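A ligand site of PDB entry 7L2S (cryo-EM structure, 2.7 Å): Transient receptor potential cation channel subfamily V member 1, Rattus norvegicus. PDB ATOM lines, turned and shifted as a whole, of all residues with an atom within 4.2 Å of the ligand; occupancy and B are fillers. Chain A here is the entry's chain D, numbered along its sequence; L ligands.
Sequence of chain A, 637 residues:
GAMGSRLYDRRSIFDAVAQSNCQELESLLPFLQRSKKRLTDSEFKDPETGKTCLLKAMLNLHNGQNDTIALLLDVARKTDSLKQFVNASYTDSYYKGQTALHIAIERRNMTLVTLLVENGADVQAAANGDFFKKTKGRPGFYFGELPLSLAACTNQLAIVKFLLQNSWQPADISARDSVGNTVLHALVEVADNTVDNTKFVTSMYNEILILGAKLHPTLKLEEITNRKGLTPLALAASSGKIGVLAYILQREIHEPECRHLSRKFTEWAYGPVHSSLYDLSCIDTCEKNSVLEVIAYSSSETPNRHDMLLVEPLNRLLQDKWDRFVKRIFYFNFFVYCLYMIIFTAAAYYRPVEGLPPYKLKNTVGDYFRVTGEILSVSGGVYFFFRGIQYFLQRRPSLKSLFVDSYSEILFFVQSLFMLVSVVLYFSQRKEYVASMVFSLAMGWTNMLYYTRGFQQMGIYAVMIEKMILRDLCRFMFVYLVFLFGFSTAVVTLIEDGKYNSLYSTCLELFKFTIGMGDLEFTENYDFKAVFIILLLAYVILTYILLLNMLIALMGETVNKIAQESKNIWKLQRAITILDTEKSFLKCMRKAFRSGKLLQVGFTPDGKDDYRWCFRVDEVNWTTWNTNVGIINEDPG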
ATOM      1  N   ARG A 305       8.536 -11.605  -8.438  1.00  0.00           N
ATOM      2  CA  ARG A 305       9.764 -12.294  -8.822  1.00  0.00           C
ATOM      3  C   ARG A 305       9.911 -13.651  -8.140  1.00  0.00           C
ATOM      4  O   ARG A 305      10.330 -14.626  -8.772  1.00  0.00           O
ATOM      5  CB  ARG A 305      10.950 -11.393  -8.494  1.00  0.00           C
ATOM      6  CG  ARG A 305      12.285 -11.931  -8.909  1.00  0.00           C
ATOM      7  CD  ARG A 305      13.328 -10.838  -8.855  1.00  0.00           C
ATOM      8  NE  ARG A 305      14.682 -11.355  -9.002  1.00  0.00           N
ATOM      9  CZ  ARG A 305      15.424 -11.874  -8.032  1.00  0.00           C
ATOM     10  NH1 ARG A 305      14.955 -11.985  -6.786  1.00  0.00           N
ATOM     11  NH2 ARG A 305      16.640 -12.312  -8.296  1.00  0.00           N
ATOM     12  N   HIS A 306       9.568 -13.726  -6.855  1.00  0.00           N
ATOM     13  CA  HIS A 306       9.710 -14.970  -6.102  1.00  0.00           C
ATOM     14  C   HIS A 306       8.502 -15.885  -6.223  1.00  0.00           C
ATOM     15  O   HIS A 306       8.650 -17.093  -5.982  1.00  0.00           O
ATOM     16  CB  HIS A 306       9.942 -14.638  -4.625  1.00  0.00           C
ATOM     17  CG  HIS A 306      11.128 -13.754  -4.397  1.00  0.00           C
ATOM     18  ND1 HIS A 306      11.017 -12.418  -4.092  1.00  0.00           N
ATOM     19  CD2 HIS A 306      12.463 -14.016  -4.453  1.00  0.00           C
ATOM     20  CE1 HIS A 306      12.210 -11.893  -3.955  1.00  0.00           C
ATOM     21  NE2 HIS A 306      13.110 -12.842  -4.178  1.00  0.00           N
ATOM     22  N   ASP A 405      21.186  -7.030  -4.162  1.00  0.00           N
ATOM     23  CA  ASP A 405      21.150  -8.389  -4.693  1.00  0.00           C
ATOM     24  C   ASP A 405      22.575  -8.894  -4.824  1.00  0.00           C
ATOM     25  O   ASP A 405      23.548  -8.138  -4.685  1.00  0.00           O
ATOM     26  CB  ASP A 405      20.418  -8.408  -6.033  1.00  0.00           C
ATOM     27  CG  ASP A 405      19.806  -9.743  -6.322  1.00  0.00           C
ATOM     28  OD1 ASP A 405      20.464 -10.763  -6.017  1.00  0.00           O
ATOM     29  OD2 ASP A 405      18.677  -9.777  -6.847  1.00  0.00           O
ATOM     30  N   TYR A 407      24.615 -11.016  -3.089  1.00  0.00           N
ATOM     31  CA  TYR A 407      25.516 -10.884  -1.948  1.00  0.00           C
ATOM     32  C   TYR A 407      26.621 -11.928  -1.984  1.00  0.00           C
ATOM     33  O   TYR A 407      27.766 -11.633  -1.638  1.00  0.00           O
ATOM     34  CB  TYR A 407      24.735 -11.016  -0.652  1.00  0.00           C
ATOM     35  CG  TYR A 407      23.678  -9.972  -0.455  1.00  0.00           C
ATOM     36  CD1 TYR A 407      24.015  -8.650  -0.228  1.00  0.00           C
ATOM     37  CD2 TYR A 407      22.347 -10.314  -0.440  1.00  0.00           C
ATOM     38  CE1 TYR A 407      23.049  -7.704  -0.031  1.00  0.00           C
ATOM     39  CE2 TYR A 407      21.372  -9.378  -0.246  1.00  0.00           C
ATOM     40  CZ  TYR A 407      21.732  -8.073  -0.036  1.00  0.00           C
ATOM     41  OH  TYR A 407      20.760  -7.134   0.171  1.00  0.00           O
ATOM     42  N   SER A 408      26.303 -13.154  -2.386  1.00  0.00           N
ATOM     43  CA  SER A 408      27.273 -14.240  -2.297  1.00  0.00           C
ATOM     44  C   SER A 408      28.418 -14.053  -3.287  1.00  0.00           C
ATOM     45  O   SER A 408      29.575 -14.370  -2.974  1.00  0.00           O
ATOM     46  CB  SER A 408      26.581 -15.575  -2.525  1.00  0.00           C
ATOM     47  OG  SER A 408      25.987 -15.634  -3.796  1.00  0.00           O
ATOM     48  N   LEU A 411      30.726 -11.550  -1.679  1.00  0.00           N
ATOM     49  CA  LEU A 411      31.493 -12.094  -0.567  1.00  0.00           C
ATOM     50  C   LEU A 411      32.631 -12.990  -1.038  1.00  0.00           C
ATOM     51  O   LEU A 411      33.760 -12.883  -0.547  1.00  0.00           O
ATOM     52  CB  LEU A 411      30.560 -12.856   0.376  1.00  0.00           C
ATOM     53  CG  LEU A 411      29.554 -11.997   1.153  1.00  0.00           C
ATOM     54  CD1 LEU A 411      28.490 -12.852   1.770  1.00  0.00           C
ATOM     55  CD2 LEU A 411      30.229 -11.167   2.222  1.00  0.00           C
ATOM     56  N   ALA A 442      38.791 -15.964   7.816  1.00  0.00           N
ATOM     57  CA  ALA A 442      37.515 -15.856   8.494  1.00  0.00           C
ATOM     58  C   ALA A 442      36.370 -15.883   7.501  1.00  0.00           C
ATOM     59  O   ALA A 442      35.419 -16.662   7.657  1.00  0.00           O
ATOM     60  CB  ALA A 442      37.470 -14.586   9.328  1.00  0.00           C
ATOM     61  N   MET A 443      36.511 -15.120   6.413  1.00  0.00           N
ATOM     62  CA  MET A 443      35.445 -15.090   5.414  1.00  0.00           C
ATOM     63  C   MET A 443      35.286 -16.442   4.772  1.00  0.00           C
ATOM     64  O   MET A 443      34.150 -16.893   4.540  1.00  0.00           O
ATOM     65  CB  MET A 443      35.746 -14.011   4.372  1.00  0.00           C
ATOM     66  CG  MET A 443      35.639 -12.607   4.924  1.00  0.00           C
ATOM     67  SD  MET A 443      35.803 -11.343   3.662  1.00  0.00           S
ATOM     68  CE  MET A 443      34.198 -11.451   2.890  1.00  0.00           C
ATOM     69  N   THR A 446      32.843 -18.503   6.818  1.00  0.00           N
ATOM     70  CA  THR A 446      31.451 -18.075   6.862  1.00  0.00           C
ATOM     71  C   THR A 446      30.777 -18.266   5.512  1.00  0.00           C
ATOM     72  O   THR A 446      29.590 -18.585   5.449  1.00  0.00           O
ATOM     73  CB  THR A 446      31.341 -16.623   7.289  1.00  0.00           C
ATOM     74  OG1 THR A 446      32.093 -15.793   6.410  1.00  0.00           O
ATOM     75  CG2 THR A 446      31.836 -16.449   8.694  1.00  0.00           C
ATOM     76  N   LEU A 449      28.455 -21.227   4.649  1.00  0.00           N
ATOM     77  CA  LEU A 449      27.009 -21.154   4.793  1.00  0.00           C
ATOM     78  C   LEU A 449      26.284 -21.102   3.448  1.00  0.00           C
ATOM     79  O   LEU A 449      25.114 -21.473   3.386  1.00  0.00           O
ATOM     80  CB  LEU A 449      26.639 -19.935   5.643  1.00  0.00           C
ATOM     81  CG  LEU A 449      25.258 -19.901   6.294  1.00  0.00           C
ATOM     82  CD1 LEU A 449      25.156 -20.915   7.421  1.00  0.00           C
ATOM     83  CD2 LEU A 449      24.968 -18.514   6.827  1.00  0.00           C
ATOM     84  N   TYR A 450      26.977 -20.664   2.378  1.00  0.00           N
ATOM     85  CA  TYR A 450      26.424 -20.695   1.028  1.00  0.00           C
ATOM     86  C   TYR A 450      25.892 -22.075   0.667  1.00  0.00           C
ATOM     87  O   TYR A 450      24.849 -22.187   0.024  1.00  0.00           O
ATOM     88  CB  TYR A 450      27.494 -20.293   0.011  1.00  0.00           C
ATOM     89  CG  TYR A 450      27.115 -20.524  -1.428  1.00  0.00           C
ATOM     90  CD1 TYR A 450      26.330 -19.615  -2.122  1.00  0.00           C
ATOM     91  CD2 TYR A 450      27.550 -21.642  -2.125  1.00  0.00           C
ATOM     92  CE1 TYR A 450      25.988 -19.821  -3.426  1.00  0.00           C
ATOM     93  CE2 TYR A 450      27.203 -21.865  -3.416  1.00  0.00           C
ATOM     94  CZ  TYR A 450      26.424 -20.943  -4.062  1.00  0.00           C
ATOM     95  OH  TYR A 450      26.073 -21.160  -5.369  1.00  0.00           O
ATOM     96  N   ARG A 453      21.970 -24.082   0.969  1.00  0.00           N
ATOM     97  CA  ARG A 453      21.045 -24.395  -0.119  1.00  0.00           C
ATOM     98  C   ARG A 453      21.458 -25.733  -0.715  1.00  0.00           C
ATOM     99  O   ARG A 453      22.635 -26.092  -0.738  1.00  0.00           O
ATOM    100  CB  ARG A 453      21.062 -23.299  -1.189  1.00  0.00           C
ATOM    101  CG  ARG A 453      22.273 -23.261  -2.106  1.00  0.00           C
ATOM    102  CD  ARG A 453      22.358 -21.974  -2.883  1.00  0.00           C
ATOM    103  NE  ARG A 453      22.728 -20.872  -2.017  1.00  0.00           N
ATOM    104  CZ  ARG A 453      22.722 -19.580  -2.343  1.00  0.00           C
ATOM    105  NH1 ARG A 453      23.076 -18.694  -1.432  1.00  0.00           N
ATOM    106  NH2 ARG A 453      22.369 -19.168  -3.555  1.00  0.00           N
ATOM    107  N   GLU A 466      19.586 -14.168   6.916  1.00  0.00           N
ATOM    108  CA  GLU A 466      19.757 -12.988   6.067  1.00  0.00           C
ATOM    109  C   GLU A 466      18.721 -11.911   6.386  1.00  0.00           C
ATOM    110  O   GLU A 466      19.059 -10.731   6.513  1.00  0.00           O
ATOM    111  CB  GLU A 466      19.647 -13.418   4.596  1.00  0.00           C
ATOM    112  CG  GLU A 466      19.539 -12.297   3.516  1.00  0.00           C
ATOM    113  CD  GLU A 466      19.061 -12.820   2.205  1.00  0.00           C
ATOM    114  OE1 GLU A 466      19.008 -14.055   2.011  1.00  0.00           O
ATOM    115  OE2 GLU A 466      18.714 -11.992   1.338  1.00  0.00           O
ATOM    116  N   LYS A 467      17.460 -12.300   6.469  1.00  0.00           N
ATOM    117  CA  LYS A 467      16.418 -11.302   6.689  1.00  0.00           C
ATOM    118  C   LYS A 467      16.503 -10.693   8.090  1.00  0.00           C
ATOM    119  O   LYS A 467      16.212  -9.511   8.253  1.00  0.00           O
ATOM    120  CB  LYS A 467      15.040 -11.910   6.445  1.00  0.00           C
ATOM    121  CG  LYS A 467      14.796 -12.375   5.013  1.00  0.00           C
ATOM    122  CD  LYS A 467      14.859 -11.255   3.999  1.00  0.00           C
ATOM    123  CE  LYS A 467      14.558 -11.736   2.610  1.00  0.00           C
ATOM    124  NZ  LYS A 467      14.828 -10.661   1.624  1.00  0.00           N
ATOM    125  N   ILE A 569      12.064 -17.718  -1.526  1.00  0.00           N
ATOM    126  CA  ILE A 569      13.405 -17.228  -1.832  1.00  0.00           C
ATOM    127  C   ILE A 569      14.397 -18.373  -1.916  1.00  0.00           C
ATOM    128  O   ILE A 569      15.290 -18.374  -2.770  1.00  0.00           O
ATOM    129  CB  ILE A 569      13.835 -16.157  -0.801  1.00  0.00           C
ATOM    130  CG1 ILE A 569      13.003 -14.887  -0.985  1.00  0.00           C
ATOM    131  CG2 ILE A 569      15.307 -15.807  -0.986  1.00  0.00           C
ATOM    132  CD1 ILE A 569      12.960 -13.976   0.201  1.00  0.00           C
ATOM    133  N   LEU A 572      14.004 -20.004  -5.314  1.00  0.00           N
ATOM    134  CA  LEU A 572      14.645 -19.228  -6.373  1.00  0.00           C
ATOM    135  C   LEU A 572      16.162 -19.382  -6.342  1.00  0.00           C
ATOM    136  O   LEU A 572      16.814 -19.426  -7.397  1.00  0.00           O
ATOM    137  CB  LEU A 572      14.240 -17.759  -6.246  1.00  0.00           C
ATOM    138  CG  LEU A 572      14.757 -16.765  -7.289  1.00  0.00           C
ATOM    139  CD1 LEU A 572      14.281 -17.122  -8.675  1.00  0.00           C
ATOM    140  CD2 LEU A 572      14.319 -15.379  -6.903  1.00  0.00           C
ATOM    141  N   GLN A 573      16.752 -19.447  -5.145  1.00  0.00           N
ATOM    142  CA  GLN A 573      18.199 -19.670  -5.038  1.00  0.00           C
ATOM    143  C   GLN A 573      18.600 -20.993  -5.657  1.00  0.00           C
ATOM    144  O   GLN A 573      19.591 -21.074  -6.404  1.00  0.00           O
ATOM    145  CB  GLN A 573      18.619 -19.642  -3.573  1.00  0.00           C
ATOM    146  CG  GLN A 573      18.678 -18.262  -2.963  1.00  0.00           C
ATOM    147  CD  GLN A 573      18.918 -18.311  -1.473  1.00  0.00           C
ATOM    148  OE1 GLN A 573      18.892 -19.368  -0.865  1.00  0.00           O
ATOM    149  NE2 GLN A 573      19.163 -17.156  -0.889  1.00  0.00           N
ATOM    150  N   ILE A 576      18.496 -20.787  -9.494  1.00  0.00           N
ATOM    151  CA  ILE A 576      19.680 -20.133 -10.063  1.00  0.00           C
ATOM    152  C   ILE A 576      20.858 -21.103 -10.079  1.00  0.00           C
ATOM    153  O   ILE A 576      21.639 -21.137 -11.037  1.00  0.00           O
ATOM    154  CB  ILE A 576      20.018 -18.840  -9.299  1.00  0.00           C
ATOM    155  CG1 ILE A 576      18.959 -17.765  -9.556  1.00  0.00           C
ATOM    156  CG2 ILE A 576      21.397 -18.316  -9.700  1.00  0.00           C
ATOM    157  CD1 ILE A 576      18.955 -16.619  -8.564  1.00  0.00           C
HETATM  158  C1  LIG L   1      26.022  -8.771   4.696  1.00  0.00           C
HETATM  159  O1  LIG L   1      19.182 -13.160  -0.743  1.00  0.00           O
HETATM  160  C2  LIG L   1      27.549 -14.021   6.929  1.00  0.00           C
HETATM  161  C3  LIG L   1      27.742 -12.563   6.525  1.00  0.00           C
HETATM  162  C4  LIG L   1      30.154 -12.304   7.247  1.00  0.00           C
HETATM  163  C5  LIG L   1      31.135 -11.233   7.704  1.00  0.00           C
HETATM  164  C6  LIG L   1      32.484 -11.876   8.001  1.00  0.00           C
HETATM  165  C7  LIG L   1      34.804 -11.417   8.788  1.00  0.00           C
HETATM  166  C8  LIG L   1      17.539 -12.632  -2.345  1.00  0.00           C
HETATM  167  C9  LIG L   1      17.828 -13.726  -4.530  1.00  0.00           C
HETATM  168  C10 LIG L   1      17.228 -12.534  -3.820  1.00  0.00           C
HETATM  169  O2  LIG L   1      17.767 -11.349  -4.320  1.00  0.00           O
HETATM  170  C11 LIG L   1      25.496 -16.025   1.632  1.00  0.00           C
HETATM  171  C12 LIG L   1      26.832 -16.146   2.351  1.00  0.00           C
HETATM  172  C13 LIG L   1      26.619 -16.165   3.864  1.00  0.00           C
HETATM  173  C14 LIG L   1      27.364 -15.044   4.610  1.00  0.00           C
HETATM  174  C15 LIG L   1      26.649 -14.755   5.937  1.00  0.00           C
HETATM  175  C16 LIG L   1      28.718 -11.832   7.443  1.00  0.00           C
HETATM  176  C17 LIG L   1      19.334 -13.733  -4.383  1.00  0.00           C
HETATM  177  C18 LIG L   1      33.509 -10.785   8.273  1.00  0.00           C
HETATM  178  C19 LIG L   1      19.038 -12.772  -2.077  1.00  0.00           C
HETATM  179  C20 LIG L   1      19.754 -13.820  -2.918  1.00  0.00           C
HETATM  180  C21 LIG L   1      22.675 -15.089   0.459  1.00  0.00           C
HETATM  181  C22 LIG L   1      23.557 -14.654   1.640  1.00  0.00           C
HETATM  182  C23 LIG L   1      23.273 -13.214   2.028  1.00  0.00           C
HETATM  183  C24 LIG L   1      23.673 -11.642   3.741  1.00  0.00           C
HETATM  184  C25 LIG L   1      24.999 -10.935   3.997  1.00  0.00           C
HETATM  185  C26 LIG L   1      24.699  -9.500   4.437  1.00  0.00           C
HETATM  186  O3  LIG L   1      17.508 -13.646  -5.885  1.00  0.00           O
HETATM  187  O4  LIG L   1      24.924 -17.012   1.332  1.00  0.00           O
HETATM  188  O5  LIG L   1      17.097 -11.463  -1.727  1.00  0.00           O
HETATM  189  O6  LIG L   1      19.835 -14.848  -5.054  1.00  0.00           O
HETATM  190  O7  LIG L   1      21.111 -13.543  -2.825  1.00  0.00           O
HETATM  191  O8  LIG L   1      21.822 -15.917  -2.183  1.00  0.00           O
HETATM  192  O9  LIG L   1      23.422 -14.562  -2.841  1.00  0.00           O
HETATM  193  O10 LIG L   1      22.493 -14.089  -0.508  1.00  0.00           O
HETATM  194  O11 LIG L   1      23.591 -12.985   3.372  1.00  0.00           O
HETATM  195  O12 LIG L   1      22.687 -11.015   3.868  1.00  0.00           O
HETATM  196  O13 LIG L   1      24.913 -14.793   1.319  1.00  0.00           O
HETATM  197  P1  LIG L   1      22.196 -14.526  -2.076  1.00  0.00           P
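O9 of the ligand is in hydrogen-bond range of N of Ser 408, at 3.2 Å.
The side-chain carboxylate of Asp 405 is in hydrogen-bond range of an oxygen (O2) of the ligand.
The side-chain carboxylate (OE2) of Glu 466 sits at hydrogen-bond distance from an oxygen (O1) of the ligand.
An oxygen (O3) of the ligand lies within hydrogen-bond range of the guanidinium group (NH2) of Arg 305.
NE2 of Gln 573 lies within hydrogen-bond range of O8 of the ligand, at 3.2 Å.
O8 of the ligand lies within salt-bridge range of NH1 of Arg 453.
O9 of the ligand lies within hydrogen-bond range of OG of Ser 408 (2.9 Å).
N of Tyr 407 touches O9 of the ligand, at 3.7 Å.
Leu 411 touches the ligand (CD1 to C12, 3.7 Å).
Tyr 450 touches the ligand.
Leu 572 touches the ligand.
Of the 18 residues printed, 10 come within 4 Å of the ligand.
The guanidinium group of Arg 305 is in salt-bridge range of the side-chain carboxylate of Asp 405.
NE of Arg 453 lies within hydrogen-bond range of O of Tyr 450.
A ring nitrogen (NE2) of His 306 lies within hydrogen-bond range of the guanidinium group of Arg 305, at 3.3 Å.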
